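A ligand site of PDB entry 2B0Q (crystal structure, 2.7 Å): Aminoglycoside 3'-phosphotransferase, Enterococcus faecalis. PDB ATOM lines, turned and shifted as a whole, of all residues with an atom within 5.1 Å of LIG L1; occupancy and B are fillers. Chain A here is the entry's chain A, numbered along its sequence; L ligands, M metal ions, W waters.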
ATOM      1  N   GLU A  23       7.203  10.793   6.864  1.00  0.00           N
ATOM      2  CA  GLU A  23       8.504  10.285   7.281  1.00  0.00           C
ATOM      3  C   GLU A  23       8.369   8.857   7.832  1.00  0.00           C
ATOM      4  O   GLU A  23       9.344   8.268   8.322  1.00  0.00           O
ATOM      5  CB  GLU A  23       9.088  11.231   8.350  1.00  0.00           C
ATOM      6  CG  GLU A  23      10.333  10.743   9.070  1.00  0.00           C
ATOM      7  CD  GLU A  23      11.558  10.708   8.195  1.00  0.00           C
ATOM      8  OE1 GLU A  23      12.001  11.785   7.762  1.00  0.00           O
ATOM      9  OE2 GLU A  23      12.079   9.605   7.935  1.00  0.00           O
ATOM     10  N   MET A  25       7.836   5.325   6.704  1.00  0.00           N
ATOM     11  CA  MET A  25       7.790   4.255   5.713  1.00  0.00           C
ATOM     12  C   MET A  25       6.981   3.039   6.178  1.00  0.00           C
ATOM     13  O   MET A  25       6.798   2.083   5.423  1.00  0.00           O
ATOM     14  CB  MET A  25       9.225   3.800   5.358  1.00  0.00           C
ATOM     15  CG  MET A  25      10.004   4.736   4.405  1.00  0.00           C
ATOM     16  SD  MET A  25      11.745   4.198   4.080  1.00  0.00           S
ATOM     17  CE  MET A  25      11.549   2.988   2.712  1.00  0.00           C
ATOM     18  N   SER A  26       6.492   3.088   7.408  1.00  0.00           N
ATOM     19  CA  SER A  26       5.720   1.993   7.972  1.00  0.00           C
ATOM     20  C   SER A  26       4.222   2.006   7.629  1.00  0.00           C
ATOM     21  O   SER A  26       3.749   2.874   6.898  1.00  0.00           O
ATOM     22  CB  SER A  26       5.888   1.983   9.487  1.00  0.00           C
ATOM     23  OG  SER A  26       4.892   2.754  10.125  1.00  0.00           O
ATOM     24  N   TYR A  54       4.156  -3.691  14.835  1.00  0.00           N
ATOM     25  CA  TYR A  54       3.860  -2.421  14.196  1.00  0.00           C
ATOM     26  C   TYR A  54       2.682  -1.847  14.950  1.00  0.00           C
ATOM     27  O   TYR A  54       2.470  -0.635  14.958  1.00  0.00           O
ATOM     28  CB  TYR A  54       3.464  -2.616  12.744  1.00  0.00           C
ATOM     29  CG  TYR A  54       4.549  -3.170  11.850  1.00  0.00           C
ATOM     30  CD1 TYR A  54       5.071  -4.446  12.045  1.00  0.00           C
ATOM     31  CD2 TYR A  54       5.025  -2.424  10.777  1.00  0.00           C
ATOM     32  CE1 TYR A  54       6.025  -4.976  11.177  1.00  0.00           C
ATOM     33  CE2 TYR A  54       5.976  -2.940   9.909  1.00  0.00           C
ATOM     34  CZ  TYR A  54       6.477  -4.213  10.112  1.00  0.00           C
ATOM     35  OH  TYR A  54       7.416  -4.717   9.234  1.00  0.00           O
ATOM     36  N   SER A  98      18.329  13.406  12.337  1.00  0.00           N
ATOM     37  CA  SER A  98      18.523  13.553  10.890  1.00  0.00           C
ATOM     38  C   SER A  98      18.458  15.011  10.472  1.00  0.00           C
ATOM     39  O   SER A  98      18.996  15.395   9.441  1.00  0.00           O
ATOM     40  CB  SER A  98      17.427  12.773  10.169  1.00  0.00           C
ATOM     41  OG  SER A  98      16.203  12.963  10.856  1.00  0.00           O
ATOM     42  N   GLU A 156      10.708  -2.902  -1.719  1.00  0.00           N
ATOM     43  CA  GLU A 156      11.376  -2.395  -0.511  1.00  0.00           C
ATOM     44  C   GLU A 156      12.747  -1.796  -0.867  1.00  0.00           C
ATOM     45  O   GLU A 156      13.179  -1.865  -2.015  1.00  0.00           O
ATOM     46  CB  GLU A 156      11.555  -3.536   0.495  1.00  0.00           C
ATOM     47  CG  GLU A 156      12.389  -3.212   1.721  1.00  0.00           C
ATOM     48  CD  GLU A 156      11.637  -2.405   2.754  1.00  0.00           C
ATOM     49  OE1 GLU A 156      10.575  -2.879   3.207  1.00  0.00           O
ATOM     50  OE2 GLU A 156      12.105  -1.299   3.121  1.00  0.00           O
ATOM     51  N   ASN A 157      13.414  -1.192   0.108  1.00  0.00           N
ATOM     52  CA  ASN A 157      14.728  -0.585  -0.114  1.00  0.00           C
ATOM     53  C   ASN A 157      15.861  -1.494   0.280  1.00  0.00           C
ATOM     54  O   ASN A 157      16.681  -1.154   1.135  1.00  0.00           O
ATOM     55  CB  ASN A 157      14.854   0.728   0.662  1.00  0.00           C
ATOM     56  CG  ASN A 157      14.276   1.914  -0.095  1.00  0.00           C
ATOM     57  OD1 ASN A 157      14.148   3.020   0.445  1.00  0.00           O
ATOM     58  ND2 ASN A 157      13.921   1.688  -1.359  1.00  0.00           N
ATOM     59  N   TRP A 158      15.918  -2.664  -0.368  1.00  0.00           N
ATOM     60  CA  TRP A 158      16.949  -3.671  -0.124  1.00  0.00           C
ATOM     61  C   TRP A 158      18.364  -3.055  -0.009  1.00  0.00           C
ATOM     62  O   TRP A 158      18.628  -1.956  -0.497  1.00  0.00           O
ATOM     63  CB  TRP A 158      16.909  -4.731  -1.227  1.00  0.00           C
ATOM     64  CG  TRP A 158      15.520  -5.003  -1.743  1.00  0.00           C
ATOM     65  CD1 TRP A 158      15.004  -4.657  -2.959  1.00  0.00           C
ATOM     66  CD2 TRP A 158      14.457  -5.654  -1.032  1.00  0.00           C
ATOM     67  NE1 TRP A 158      13.697  -5.049  -3.054  1.00  0.00           N
ATOM     68  CE2 TRP A 158      13.330  -5.660  -1.890  1.00  0.00           C
ATOM     69  CE3 TRP A 158      14.341  -6.223   0.236  1.00  0.00           C
ATOM     70  CZ2 TRP A 158      12.109  -6.222  -1.510  1.00  0.00           C
ATOM     71  CZ3 TRP A 158      13.120  -6.785   0.615  1.00  0.00           C
ATOM     72  CH2 TRP A 158      12.025  -6.777  -0.264  1.00  0.00           C
ATOM     73  N   GLU A 159      19.265  -3.799   0.619  1.00  0.00           N
ATOM     74  CA  GLU A 159      20.622  -3.334   0.876  1.00  0.00           C
ATOM     75  C   GLU A 159      21.727  -3.514  -0.163  1.00  0.00           C
ATOM     76  O   GLU A 159      22.886  -3.328   0.171  1.00  0.00           O
ATOM     77  CB  GLU A 159      21.116  -3.939   2.201  1.00  0.00           C
ATOM     78  CG  GLU A 159      20.576  -3.236   3.426  1.00  0.00           C
ATOM     79  CD  GLU A 159      21.374  -1.999   3.794  1.00  0.00           C
ATOM     80  OE1 GLU A 159      20.779  -1.030   4.331  1.00  0.00           O
ATOM     81  OE2 GLU A 159      22.606  -2.006   3.563  1.00  0.00           O
ATOM     82  N   ASP A 189      14.591  -0.390  16.059  1.00  0.00           N
ATOM     83  CA  ASP A 189      14.549   0.442  14.859  1.00  0.00           C
ATOM     84  C   ASP A 189      15.364   1.707  15.103  1.00  0.00           C
ATOM     85  O   ASP A 189      14.886   2.819  14.858  1.00  0.00           O
ATOM     86  CB  ASP A 189      13.106   0.812  14.541  1.00  0.00           C
ATOM     87  CG  ASP A 189      12.924   1.258  13.129  1.00  0.00           C
ATOM     88  OD1 ASP A 189      13.940   1.617  12.479  1.00  0.00           O
ATOM     89  OD2 ASP A 189      11.756   1.245  12.660  1.00  0.00           O
ATOM     90  N   ASP A 192      18.435   7.528  12.719  1.00  0.00           N
ATOM     91  CA  ASP A 192      18.306   8.986  12.861  1.00  0.00           C
ATOM     92  C   ASP A 192      16.890   9.532  12.718  1.00  0.00           C
ATOM     93  O   ASP A 192      16.627  10.663  13.117  1.00  0.00           O
ATOM     94  CB  ASP A 192      19.242   9.709  11.880  1.00  0.00           C
ATOM     95  CG  ASP A 192      18.911   9.440  10.421  1.00  0.00           C
ATOM     96  OD1 ASP A 192      17.733   9.576  10.022  1.00  0.00           O
ATOM     97  OD2 ASP A 192      19.831   9.089   9.649  1.00  0.00           O
ATOM     98  N   SER A 193      15.996   8.739  12.155  1.00  0.00           N
ATOM     99  CA  SER A 193      14.603   9.153  11.947  1.00  0.00           C
ATOM    100  C   SER A 193      13.761   8.907  13.204  1.00  0.00           C
ATOM    101  O   SER A 193      12.710   9.529  13.402  1.00  0.00           O
ATOM    102  CB  SER A 193      14.026   8.376  10.759  1.00  0.00           C
ATOM    103  OG  SER A 193      12.629   8.507  10.630  1.00  0.00           O
ATOM    104  N   ASN A 194      14.243   8.003  14.056  1.00  0.00           N
ATOM    105  CA  ASN A 194      13.532   7.690  15.275  1.00  0.00           C
ATOM    106  C   ASN A 194      14.266   8.152  16.529  1.00  0.00           C
ATOM    107  O   ASN A 194      13.841   7.819  17.621  1.00  0.00           O
ATOM    108  CB  ASN A 194      13.251   6.190  15.350  1.00  0.00           C
ATOM    109  CG  ASN A 194      12.578   5.661  14.102  1.00  0.00           C
ATOM    110  OD1 ASN A 194      11.584   6.232  13.631  1.00  0.00           O
ATOM    111  ND2 ASN A 194      13.099   4.584  13.562  1.00  0.00           N
ATOM    112  N   ASP A 207       9.076   5.669  17.955  1.00  0.00           N
ATOM    113  CA  ASP A 207       8.973   4.499  17.088  1.00  0.00           C
ATOM    114  C   ASP A 207       9.430   3.302  17.935  1.00  0.00           C
ATOM    115  O   ASP A 207      10.478   2.695  17.661  1.00  0.00           O
ATOM    116  CB  ASP A 207       9.893   4.674  15.869  1.00  0.00           C
ATOM    117  CG  ASP A 207       9.319   4.072  14.593  1.00  0.00           C
ATOM    118  OD1 ASP A 207       8.478   3.151  14.687  1.00  0.00           O
ATOM    119  OD2 ASP A 207       9.725   4.510  13.490  1.00  0.00           O
ATOM    120  N   ARG A 210       9.167  -2.396  18.166  1.00  0.00           N
ATOM    121  CA  ARG A 210       9.995  -3.574  18.388  1.00  0.00           C
ATOM    122  C   ARG A 210      10.914  -3.385  19.570  1.00  0.00           C
ATOM    123  O   ARG A 210      11.930  -4.061  19.696  1.00  0.00           O
ATOM    124  CB  ARG A 210      10.834  -3.856  17.153  1.00  0.00           C
ATOM    125  CG  ARG A 210      10.004  -4.157  15.968  1.00  0.00           C
ATOM    126  CD  ARG A 210      10.819  -4.061  14.721  1.00  0.00           C
ATOM    127  NE  ARG A 210       9.943  -4.018  13.550  1.00  0.00           N
ATOM    128  CZ  ARG A 210      10.244  -3.357  12.446  1.00  0.00           C
ATOM    129  NH1 ARG A 210      11.388  -2.699  12.365  1.00  0.00           N
ATOM    130  NH2 ARG A 210       9.390  -3.349  11.440  1.00  0.00           N
ATOM    131  N   ARG A 225      24.748  -0.158   9.797  1.00  0.00           N
ATOM    132  CA  ARG A 225      24.003   0.035   8.551  1.00  0.00           C
ATOM    133  C   ARG A 225      23.865   1.512   8.223  1.00  0.00           C
ATOM    134  O   ARG A 225      24.230   1.956   7.136  1.00  0.00           O
ATOM    135  CB  ARG A 225      22.608  -0.595   8.649  1.00  0.00           C
ATOM    136  CG  ARG A 225      21.867  -0.638   7.334  1.00  0.00           C
ATOM    137  CD  ARG A 225      20.518  -1.295   7.462  1.00  0.00           C
ATOM    138  NE  ARG A 225      19.587  -0.499   8.266  1.00  0.00           N
ATOM    139  CZ  ARG A 225      18.322  -0.859   8.509  1.00  0.00           C
ATOM    140  NH1 ARG A 225      17.539  -0.090   9.245  1.00  0.00           N
ATOM    141  NH2 ARG A 225      17.849  -2.001   8.010  1.00  0.00           N
ATOM    142  N   GLU A 229      25.882   3.533   5.024  1.00  0.00           N
ATOM    143  CA  GLU A 229      25.147   4.143   3.930  1.00  0.00           C
ATOM    144  C   GLU A 229      25.136   5.671   3.918  1.00  0.00           C
ATOM    145  O   GLU A 229      25.063   6.278   2.857  1.00  0.00           O
ATOM    146  CB  GLU A 229      23.710   3.644   3.938  1.00  0.00           C
ATOM    147  CG  GLU A 229      22.819   4.446   4.878  1.00  0.00           C
ATOM    148  CD  GLU A 229      21.396   3.934   4.914  1.00  0.00           C
ATOM    149  OE1 GLU A 229      20.922   3.414   3.869  1.00  0.00           O
ATOM    150  OE2 GLU A 229      20.743   4.068   5.971  1.00  0.00           O
ATOM    151  N   ASP A 230      25.179   6.290   5.099  1.00  0.00           N
ATOM    152  CA  ASP A 230      25.124   7.748   5.232  1.00  0.00           C
ATOM    153  C   ASP A 230      26.443   8.497   5.305  1.00  0.00           C
ATOM    154  O   ASP A 230      26.466   9.702   5.089  1.00  0.00           O
ATOM    155  CB  ASP A 230      24.265   8.134   6.439  1.00  0.00           C
ATOM    156  CG  ASP A 230      22.784   7.947   6.188  1.00  0.00           C
ATOM    157  OD1 ASP A 230      22.003   7.905   7.169  1.00  0.00           O
ATOM    158  OD2 ASP A 230      22.399   7.851   4.996  1.00  0.00           O
ATOM    159  N   ASP A 260      16.275  -7.364   9.123  1.00  0.00           N
ATOM    160  CA  ASP A 260      15.455  -6.177   8.941  1.00  0.00           C
ATOM    161  C   ASP A 260      15.005  -5.958   7.497  1.00  0.00           C
ATOM    162  O   ASP A 260      14.115  -5.146   7.228  1.00  0.00           O
ATOM    163  CB  ASP A 260      16.225  -4.939   9.399  1.00  0.00           C
ATOM    164  CG  ASP A 260      15.308  -3.773   9.751  1.00  0.00           C
ATOM    165  OD1 ASP A 260      15.539  -2.665   9.215  1.00  0.00           O
ATOM    166  OD2 ASP A 260      14.370  -3.975  10.553  1.00  0.00           O
ATOM    167  N   GLU A 261      15.596  -6.698   6.575  1.00  0.00           N
ATOM    168  CA  GLU A 261      15.277  -6.569   5.164  1.00  0.00           C
ATOM    169  C   GLU A 261      13.789  -6.655   4.808  1.00  0.00           C
ATOM    170  O   GLU A 261      13.323  -5.921   3.932  1.00  0.00           O
ATOM    171  CB  GLU A 261      16.052  -7.605   4.356  1.00  0.00           C
ATOM    172  CG  GLU A 261      16.510  -7.067   3.019  1.00  0.00           C
ATOM    173  CD  GLU A 261      17.439  -5.887   3.186  1.00  0.00           C
ATOM    174  OE1 GLU A 261      17.191  -5.055   4.085  1.00  0.00           O
ATOM    175  OE2 GLU A 261      18.397  -5.768   2.417  1.00  0.00           O
ATOM    176  N   PHE A 263      11.185  -6.248   7.113  1.00  0.00           N
ATOM    177  CA  PHE A 263      10.293  -5.496   7.994  1.00  0.00           C
ATOM    178  C   PHE A 263      10.086  -4.045   7.541  1.00  0.00           C
ATOM    179  O   PHE A 263       9.046  -3.445   7.895  1.00  0.00           O
ATOM    180  CB  PHE A 263      10.808  -5.522   9.434  1.00  0.00           C
ATOM    181  CG  PHE A 263      10.653  -6.854  10.121  1.00  0.00           C
ATOM    182  CD1 PHE A 263      11.662  -7.804  10.070  1.00  0.00           C
ATOM    183  CD2 PHE A 263       9.481  -7.159  10.823  1.00  0.00           C
ATOM    184  CE1 PHE A 263      11.519  -9.040  10.702  1.00  0.00           C
ATOM    185  CE2 PHE A 263       9.331  -8.389  11.450  1.00  0.00           C
ATOM    186  CZ  PHE A 263      10.351  -9.329  11.398  1.00  0.00           C
ATOM    187  OXT PHE A 263      10.989  -3.520   6.850  1.00  0.00           O
HETATM  188  C1  LIG L   1      12.781   1.394   6.814  1.00  0.00           C
HETATM  189  O1  LIG L   1      13.513   0.175   7.042  1.00  0.00           O
HETATM  190  C2  LIG L   1      12.619   2.186   8.128  1.00  0.00           C
HETATM  191  N1  LIG L   1      13.929   2.130   8.854  1.00  0.00           N
HETATM  192  C3  LIG L   1      11.596   1.612   9.095  1.00  0.00           C
HETATM  193  O2  LIG L   1      11.236   2.644   9.994  1.00  0.00           O
HETATM  194  C4  LIG L   1      10.342   1.138   8.379  1.00  0.00           C
HETATM  195  O3  LIG L   1       9.539   0.407   9.309  1.00  0.00           O
HETATM  196  C5  LIG L   1      10.726   0.216   7.232  1.00  0.00           C
HETATM  197  O4  LIG L   1      11.517   0.945   6.273  1.00  0.00           O
HETATM  198  C6  LIG L   1       9.483  -0.292   6.520  1.00  0.00           C
HETATM  199  C7  LIG L   1      16.712  -1.506   4.907  1.00  0.00           C
HETATM  200  N2  LIG L   1      17.535  -2.023   3.781  1.00  0.00           N
HETATM  201  C8  LIG L   1      16.460  -0.031   4.650  1.00  0.00           C
HETATM  202  C9  LIG L   1      15.608   0.552   5.790  1.00  0.00           C
HETATM  203  O5  LIG L   1      15.385   1.939   5.513  1.00  0.00           O
HETATM  204  C10 LIG L   1      14.233  -0.189   5.869  1.00  0.00           C
HETATM  205  C11 LIG L   1      14.444  -1.727   5.962  1.00  0.00           C
HETATM  206  N3  LIG L   1      13.111  -2.354   5.739  1.00  0.00           N
HETATM  207  C12 LIG L   1      15.382  -2.272   4.864  1.00  0.00           C
HETATM  208  C13 LIG L   1      16.373   2.742   6.211  1.00  0.00           C
HETATM  209  C14 LIG L   1      16.815   3.848   5.290  1.00  0.00           C
HETATM  210  C15 LIG L   1      16.109   5.076   5.797  1.00  0.00           C
HETATM  211  C16 LIG L   1      15.709   4.707   7.207  1.00  0.00           C
HETATM  212  O6  LIG L   1      15.629   3.290   7.281  1.00  0.00           O
HETATM  213  C17 LIG L   1      14.371   5.297   7.549  1.00  0.00           C
HETATM  214  C18 LIG L   1      17.505   9.658   5.775  1.00  0.00           C
HETATM  215  C19 LIG L   1      18.544   8.595   5.460  1.00  0.00           C
HETATM  216  C20 LIG L   1      18.044   7.739   4.323  1.00  0.00           C
HETATM  217  C21 LIG L   1      16.748   7.031   4.735  1.00  0.00           C
HETATM  218  O7  LIG L   1      16.992   6.176   5.865  1.00  0.00           O
HETATM  219  C22 LIG L   1      16.137   9.044   6.131  1.00  0.00           C
HETATM  220  O8  LIG L   1      15.719   7.956   5.225  1.00  0.00           O
HETATM  221  C23 LIG L   1      16.080   8.528   7.567  1.00  0.00           C
HETATM  222  N4  LIG L   1      10.010  -0.931   5.267  1.00  0.00           N
HETATM  223  O9  LIG L   1      18.232   4.009   5.449  1.00  0.00           O
HETATM  224  O10 LIG L   1      19.737   9.239   5.055  1.00  0.00           O
HETATM  225  O11 LIG L   1      17.983  10.438   6.870  1.00  0.00           O
HETATM  226  O12 LIG L   1      14.470   5.839   8.864  1.00  0.00           O
HETATM  227  O13 LIG L   1      17.716   0.634   4.603  1.00  0.00           O
HETATM  228  N5  LIG L   1      14.621   8.568   7.887  1.00  0.00           N
HETATM  229  N6  LIG L   1      19.062   6.671   4.103  1.00  0.00           N
HETATM  230  P1  LG2 L   2       7.192   5.138  11.517  1.00  0.00           P
HETATM  231  O1  LG2 L   2       7.185   3.983  12.452  1.00  0.00           O
HETATM  232  O2  LG2 L   2       6.409   5.056  10.284  1.00  0.00           O
HETATM  233  O3  LG2 L   2       8.717   5.495  11.122  1.00  0.00           O
HETATM  234  P2  LG2 L   2       7.474   7.142  13.525  1.00  0.00           P
HETATM  235  O4  LG2 L   2       6.894   6.689  14.794  1.00  0.00           O
HETATM  236  O5  LG2 L   2       8.907   7.002  13.273  1.00  0.00           O
HETATM  237  O6  LG2 L   2       6.689   6.424  12.320  1.00  0.00           O
HETATM  238  O7  LG2 L   2       7.050   8.669  13.317  1.00  0.00           O
HETATM  239  C1  LG2 L   2       7.103   9.261  12.015  1.00  0.00           C
HETATM  240  C2  LG2 L   2       7.857  10.589  12.056  1.00  0.00           C
HETATM  241  O8  LG2 L   2       7.057  11.616  12.669  1.00  0.00           O
HETATM  242  C3  LG2 L   2       9.131  10.567  12.902  1.00  0.00           C
HETATM  243  O9  LG2 L   2      10.258  10.367  12.046  1.00  0.00           O
HETATM  244  C4  LG2 L   2       9.143  11.997  13.446  1.00  0.00           C
HETATM  245  O10 LG2 L   2       9.595  12.883  12.409  1.00  0.00           O
HETATM  246  C5  LG2 L   2       7.679  12.325  13.724  1.00  0.00           C
HETATM  247  N1  LG2 L   2       7.215  11.980  15.100  1.00  0.00           N
HETATM  248  C6  LG2 L   2       6.491  10.889  15.536  1.00  0.00           C
HETATM  249  N2  LG2 L   2       6.242  10.878  16.821  1.00  0.00           N
HETATM  250  C7  LG2 L   2       6.843  12.038  17.270  1.00  0.00           C
HETATM  251  C8  LG2 L   2       6.960  12.642  18.559  1.00  0.00           C
HETATM  252  N3  LG2 L   2       6.441  12.117  19.653  1.00  0.00           N
HETATM  253  N4  LG2 L   2       7.643  13.810  18.650  1.00  0.00           N
HETATM  254  C9  LG2 L   2       8.180  14.368  17.554  1.00  0.00           C
HETATM  255  N5  LG2 L   2       8.143  13.903  16.295  1.00  0.00           N
HETATM  256  C10 LG2 L   2       7.450  12.717  16.235  1.00  0.00           C
HETATM  257 MG    MG M   1       8.438   2.125  12.753  1.00  0.00          MG
HETATM  258 MG    MG M   2      10.511   7.118  11.783  1.00  0.00          MG
HETATM  259  O   HOH W   1      11.244   5.004  11.501  1.00  0.00           O
HETATM  260  O   HOH W   2       8.801   2.812  10.793  1.00  0.00           O
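OE2 of Glu 229 is in salt-bridge range of N6 of LIG L1 (3.6 Å).
OXT of Phe 263 lies within salt-bridge range of N3 of LIG L1 (2.7 Å).
The side-chain carboxylate (OE2) of Glu 23 lies within salt-bridge range of a nitrogen (N5) of LIG L1.
N4 of LIG L1 is in salt-bridge range of OE1 of Glu 156 (2.9 Å).
O of Asn 157 lies within hydrogen-bond range of N2 of LIG L1, 2.9 Å away.
A nitrogen (N5) of LIG L1 sits close to the side-chain hydroxyl of Ser 193.
OD2 of Asp 230 is in salt-bridge range of N6 of LIG L1 (3.7 Å).
OD1 of Asp 189 is in salt-bridge range of N1 of LIG L1, at 3.7 Å.
The side-chain carboxylate (OE1) of Glu 261 is in salt-bridge range of a nitrogen (N2) of LIG L1 (3.1 Å).
OD1 of Asp 192 lies within salt-bridge range of N5 of LIG L1 (3.9 Å).
OE1 of Glu 159 is in salt-bridge range of N2 of LIG L1, 3.4 Å away.
N3 of LIG L1 lies within hydrogen-bond range of O of Asp 260, at 3.3 Å.
O9 of LG2 L2 sits at hydrogen-bond distance from O of Ser 193 (2.9 Å).
The side-chain hydroxyl of Ser 193 lies within hydrogen-bond range of an oxygen (O9) of LG2 L2, 3.3 Å away.
An oxygen (O2) of LG2 L2 sits close to the backbone NH of Ser 26, 3.5 Å away.
The side-chain hydroxyl (OG) of Ser 26 lies within hydrogen-bond range of an oxygen (O2) of LG2 L2 (2.8 Å).
The chain-end carboxylate (O) of Phe 263 is in salt-bridge range of the guanidinium group (NH2) of Arg 210 (3.6 Å).
O of Phe 263 sits at hydrogen-bond distance from OH of Tyr 54 (2.5 Å).
OG of Ser 193 is in hydrogen-bond range of OE2 of Glu 23.
The side-chain carboxylate of Asp 189 lies within salt-bridge range of the guanidinium group of Arg 210 (3.97 Å).
N of Glu 159 sits at hydrogen-bond distance from OE2 of Glu 261 (2.8 Å).
The backbone carbonyl oxygen (O) of Asp 192 lies within hydrogen-bond range of the side-chain hydroxyl (OG) of Ser 98, at 3.3 Å.
OD1 of Asp 260 lies within salt-bridge range of NH2 of Arg 225, at 2.7 Å.
The side-chain carboxylate (OD2) of Asp 260 is in salt-bridge range of the guanidinium group (NH1) of Arg 210, at 3.7 Å.
Met 25 touches LIG L1.
Ser 26 touches LIG L1.
Arg 225 touches LIG L1.
Within 4 Å of LIG L1: Glu 23, Met 25, Ser 26, Glu 156, Asn 157, Glu 159, Asp 189, Asp 192, Ser 193, Arg 225, Glu 229, Asp 230, Asp 260, Glu 261 and Phe 263.
Along chain A the residues within 4 Å of LIG L1 span positions 23 to 263.
Water W2 lies within hydrogen-bond range of an oxygen (O2) of LIG L1 (2.6 Å), the side-chain carboxylate of Asp 207 (3.3 Å) and an oxygen (O2) of LG2 L2 (3.3 Å).
Water W1 lies within hydrogen-bond range of OD2 of Asp 207 (2.6 Å), O2 of LIG L1 (2.8 Å) and ND2 of Asn 194 (2.8 Å).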
